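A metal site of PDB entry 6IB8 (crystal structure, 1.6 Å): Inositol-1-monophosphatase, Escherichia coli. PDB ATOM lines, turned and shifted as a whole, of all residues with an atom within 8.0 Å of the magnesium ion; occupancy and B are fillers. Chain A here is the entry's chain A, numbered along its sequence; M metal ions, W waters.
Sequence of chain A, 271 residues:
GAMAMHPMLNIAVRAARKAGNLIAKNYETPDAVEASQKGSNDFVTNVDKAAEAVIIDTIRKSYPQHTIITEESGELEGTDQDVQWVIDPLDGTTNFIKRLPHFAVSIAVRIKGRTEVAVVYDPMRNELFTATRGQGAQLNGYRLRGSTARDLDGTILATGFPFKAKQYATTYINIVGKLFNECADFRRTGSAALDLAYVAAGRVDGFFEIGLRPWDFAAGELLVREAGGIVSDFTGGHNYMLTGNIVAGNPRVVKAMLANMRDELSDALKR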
ATOM      1  N   ASP A  48     -29.580  -5.371  -9.953  1.00  0.00           N
ATOM      2  CA  ASP A  48     -28.904  -4.209  -9.385  1.00  0.00           C
ATOM      3  C   ASP A  48     -27.853  -3.654 -10.346  1.00  0.00           C
ATOM      4  O   ASP A  48     -27.696  -2.438 -10.481  1.00  0.00           O
ATOM      5  CB  ASP A  48     -28.203  -4.539  -8.065  1.00  0.00           C
ATOM      6  CG  ASP A  48     -29.152  -4.973  -6.981  1.00  0.00           C
ATOM      7  OD1 ASP A  48     -29.844  -5.988  -7.148  1.00  0.00           O
ATOM      8  OD2 ASP A  48     -29.190  -4.276  -5.943  1.00  0.00           O
ATOM      9  N   GLU A  71     -22.555   1.036  -4.487  1.00  0.00           N
ATOM     10  CA  GLU A  71     -22.155  -0.158  -3.742  1.00  0.00           C
ATOM     11  C   GLU A  71     -21.568  -1.231  -4.647  1.00  0.00           C
ATOM     12  O   GLU A  71     -20.570  -1.871  -4.274  1.00  0.00           O
ATOM     13  CB  GLU A  71     -23.324  -0.713  -2.893  1.00  0.00           C
ATOM     14  CG  GLU A  71     -24.434  -1.571  -3.528  1.00  0.00           C
ATOM     15  CD  GLU A  71     -25.572  -1.917  -2.544  1.00  0.00           C
ATOM     16  OE1 GLU A  71     -25.379  -2.795  -1.691  1.00  0.00           O
ATOM     17  OE2 GLU A  71     -26.675  -1.317  -2.630  1.00  0.00           O
ATOM     18  N   GLU A  72     -22.091  -1.395  -5.870  1.00  0.00           N
ATOM     19  CA  GLU A  72     -21.568  -2.408  -6.772  1.00  0.00           C
ATOM     20  C   GLU A  72     -20.192  -2.051  -7.328  1.00  0.00           C
ATOM     21  O   GLU A  72     -19.434  -2.971  -7.668  1.00  0.00           O
ATOM     22  CB  GLU A  72     -22.530  -2.686  -7.933  1.00  0.00           C
ATOM     23  CG  GLU A  72     -24.019  -2.961  -7.588  1.00  0.00           C
ATOM     24  CD  GLU A  72     -24.227  -4.092  -6.595  1.00  0.00           C
ATOM     25  OE1 GLU A  72     -23.508  -5.101  -6.710  1.00  0.00           O
ATOM     26  OE2 GLU A  72     -25.125  -3.978  -5.704  1.00  0.00           O
ATOM     27  N   ILE A  87     -25.249   6.779  -5.191  1.00  0.00           N
ATOM     28  CA  ILE A  87     -26.307   6.020  -5.858  1.00  0.00           C
ATOM     29  C   ILE A  87     -26.551   4.688  -5.178  1.00  0.00           C
ATOM     30  O   ILE A  87     -25.591   3.925  -4.972  1.00  0.00           O
ATOM     31  CB  ILE A  87     -25.929   5.712  -7.336  1.00  0.00           C
ATOM     32  CG1 ILE A  87     -25.444   6.943  -8.092  1.00  0.00           C
ATOM     33  CG2 ILE A  87     -27.077   4.953  -8.063  1.00  0.00           C
ATOM     34  CD1 ILE A  87     -26.436   7.934  -8.228  1.00  0.00           C
ATOM     35  N   ASP A  88     -27.836   4.377  -4.874  1.00  0.00           N
ATOM     36  CA  ASP A  88     -28.258   2.995  -4.628  1.00  0.00           C
ATOM     37  C   ASP A  88     -29.168   2.573  -5.777  1.00  0.00           C
ATOM     38  O   ASP A  88     -30.316   3.056  -5.870  1.00  0.00           O
ATOM     39  CB  ASP A  88     -28.984   2.810  -3.275  1.00  0.00           C
ATOM     40  CG  ASP A  88     -29.158   1.351  -2.896  1.00  0.00           C
ATOM     41  OD1 ASP A  88     -29.090   0.494  -3.801  1.00  0.00           O
ATOM     42  OD2 ASP A  88     -29.342   1.058  -1.709  1.00  0.00           O
ATOM     43  N   PRO A  89     -28.707   1.702  -6.691  1.00  0.00           N
ATOM     44  CA  PRO A  89     -29.517   1.390  -7.869  1.00  0.00           C
ATOM     45  C   PRO A  89     -30.777   0.596  -7.565  1.00  0.00           C
ATOM     46  O   PRO A  89     -31.747   0.703  -8.316  1.00  0.00           O
ATOM     47  CB  PRO A  89     -28.537   0.579  -8.762  1.00  0.00           C
ATOM     48  CG  PRO A  89     -27.560  -0.012  -7.809  1.00  0.00           C
ATOM     49  CD  PRO A  89     -27.365   1.060  -6.724  1.00  0.00           C
ATOM     50  N   LEU A  90     -30.798  -0.146  -6.445  1.00  0.00           N
ATOM     51  CA  LEU A  90     -32.002  -0.893  -6.022  1.00  0.00           C
ATOM     52  C   LEU A  90     -31.909  -1.013  -4.499  1.00  0.00           C
ATOM     53  O   LEU A  90     -31.140  -1.841  -3.991  1.00  0.00           O
ATOM     54  CB  LEU A  90     -32.054  -2.266  -6.687  1.00  0.00           C
ATOM     55  CG  LEU A  90     -33.212  -3.213  -6.314  1.00  0.00           C
ATOM     56  CD1 LEU A  90     -34.525  -2.508  -6.313  1.00  0.00           C
ATOM     57  CD2 LEU A  90     -33.266  -4.381  -7.311  1.00  0.00           C
ATOM     58  N   ASP A  91     -32.619  -0.143  -3.776  1.00  0.00           N
ATOM     59  CA  ASP A  91     -32.708  -0.256  -2.329  1.00  0.00           C
ATOM     60  C   ASP A  91     -33.875  -1.160  -1.961  1.00  0.00           C
ATOM     61  O   ASP A  91     -35.032  -0.838  -2.248  1.00  0.00           O
ATOM     62  CB  ASP A  91     -32.881   1.116  -1.686  1.00  0.00           C
ATOM     63  CG  ASP A  91     -32.890   1.045  -0.185  1.00  0.00           C
ATOM     64  OD1 ASP A  91     -32.009   0.358   0.336  1.00  0.00           O
ATOM     65  OD2 ASP A  91     -33.793   1.599   0.446  1.00  0.00           O
ATOM     66  N   GLY A  92     -33.579  -2.292  -1.307  1.00  0.00           N
ATOM     67  CA  GLY A  92     -34.620  -3.283  -1.038  1.00  0.00           C
ATOM     68  C   GLY A  92     -34.428  -4.588  -1.796  1.00  0.00           C
ATOM     69  O   GLY A  92     -35.398  -5.171  -2.288  1.00  0.00           O
ATOM     70  N   THR A  93     -33.180  -5.082  -1.848  1.00  0.00           N
ATOM     71  CA  THR A  93     -32.862  -6.245  -2.678  1.00  0.00           C
ATOM     72  C   THR A  93     -33.628  -7.495  -2.234  1.00  0.00           C
ATOM     73  O   THR A  93     -34.161  -8.236  -3.064  1.00  0.00           O
ATOM     74  CB  THR A  93     -31.355  -6.485  -2.662  1.00  0.00           C
ATOM     75  OG1 THR A  93     -30.684  -5.311  -3.139  1.00  0.00           O
ATOM     76  CG2 THR A  93     -30.993  -7.650  -3.580  1.00  0.00           C
ATOM     77  N   ALA A 104     -36.790   0.804  -4.129  1.00  0.00           N
ATOM     78  CA  ALA A 104     -36.645   2.148  -4.695  1.00  0.00           C
ATOM     79  C   ALA A 104     -35.256   2.366  -5.310  1.00  0.00           C
ATOM     80  O   ALA A 104     -34.283   1.698  -4.935  1.00  0.00           O
ATOM     81  CB  ALA A 104     -36.858   3.263  -3.631  1.00  0.00           C
ATOM     82  N   LYS A 164     -27.042  -7.144   8.824  1.00  0.00           N
ATOM     83  CA  LYS A 164     -25.663  -7.137   8.337  1.00  0.00           C
ATOM     84  C   LYS A 164     -24.654  -6.975   9.455  1.00  0.00           C
ATOM     85  O   LYS A 164     -23.442  -6.940   9.176  1.00  0.00           O
ATOM     86  CB  LYS A 164     -25.443  -6.013   7.310  1.00  0.00           C
ATOM     87  CG  LYS A 164     -26.282  -6.081   6.038  1.00  0.00           C
ATOM     88  CD  LYS A 164     -26.000  -4.844   5.164  1.00  0.00           C
ATOM     89  CE  LYS A 164     -26.869  -4.835   3.931  1.00  0.00           C
ATOM     90  NZ  LYS A 164     -26.574  -3.654   3.069  1.00  0.00           N
ATOM     91  N   TRP A 215     -24.939   5.402   0.484  1.00  0.00           N
ATOM     92  CA  TRP A 215     -25.943   5.392  -0.571  1.00  0.00           C
ATOM     93  C   TRP A 215     -27.323   5.013  -0.075  1.00  0.00           C
ATOM     94  O   TRP A 215     -28.306   5.317  -0.778  1.00  0.00           O
ATOM     95  CB  TRP A 215     -25.544   4.423  -1.707  1.00  0.00           C
ATOM     96  CG  TRP A 215     -24.904   3.152  -1.200  1.00  0.00           C
ATOM     97  CD1 TRP A 215     -25.546   2.029  -0.696  1.00  0.00           C
ATOM     98  CD2 TRP A 215     -23.500   2.859  -1.135  1.00  0.00           C
ATOM     99  NE1 TRP A 215     -24.613   1.080  -0.322  1.00  0.00           N
ATOM    100  CE2 TRP A 215     -23.352   1.582  -0.568  1.00  0.00           C
ATOM    101  CE3 TRP A 215     -22.343   3.576  -1.504  1.00  0.00           C
ATOM    102  CZ2 TRP A 215     -22.093   0.995  -0.356  1.00  0.00           C
ATOM    103  CZ3 TRP A 215     -21.096   2.996  -1.289  1.00  0.00           C
ATOM    104  CH2 TRP A 215     -20.988   1.717  -0.742  1.00  0.00           C
ATOM    105  N   ASP A 216     -27.439   4.324   1.078  1.00  0.00           N
ATOM    106  CA  ASP A 216     -28.759   3.989   1.639  1.00  0.00           C
ATOM    107  C   ASP A 216     -29.572   5.246   2.002  1.00  0.00           C
ATOM    108  O   ASP A 216     -30.803   5.288   1.811  1.00  0.00           O
ATOM    109  CB  ASP A 216     -28.602   3.113   2.917  1.00  0.00           C
ATOM    110  CG  ASP A 216     -27.962   1.742   2.638  1.00  0.00           C
ATOM    111  OD1 ASP A 216     -28.105   1.182   1.527  1.00  0.00           O
ATOM    112  OD2 ASP A 216     -27.338   1.217   3.574  1.00  0.00           O
HETATM  113 MG    MG M   1     -28.869  -1.611  -3.058  1.00  0.00          MG
HETATM  114  O   HOH W   1     -28.770  -3.549  -2.497  1.00  0.00           O
HETATM  115  O   HOH W   2     -28.192  -2.250  -5.088  1.00  0.00           O
HETATM  116  O   HOH W   3     -29.505  -1.721  -0.974  1.00  0.00           O
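The magnesium ion is bound by water W1, water W3, water W2, the side-chain carboxylate (OD1) of Asp 88, the side-chain carboxylate (OE2) of Glu 71 and the backbone carbonyl oxygen (O) of Leu 90.
Asp 48 touches the magnesium ion (OD2 to MG, 3.9 Å).
Of the 14 residues printed, 4 come within 4 Å of the magnesium ion.
The nearest printed residue that does not touch the magnesium ion is Asp 91 (4.1 Å).
The side-chain carboxylate (OD2) of Asp 48 sits at hydrogen-bond distance from the side-chain hydroxyl (OG1) of Thr 93 (3.3 Å).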
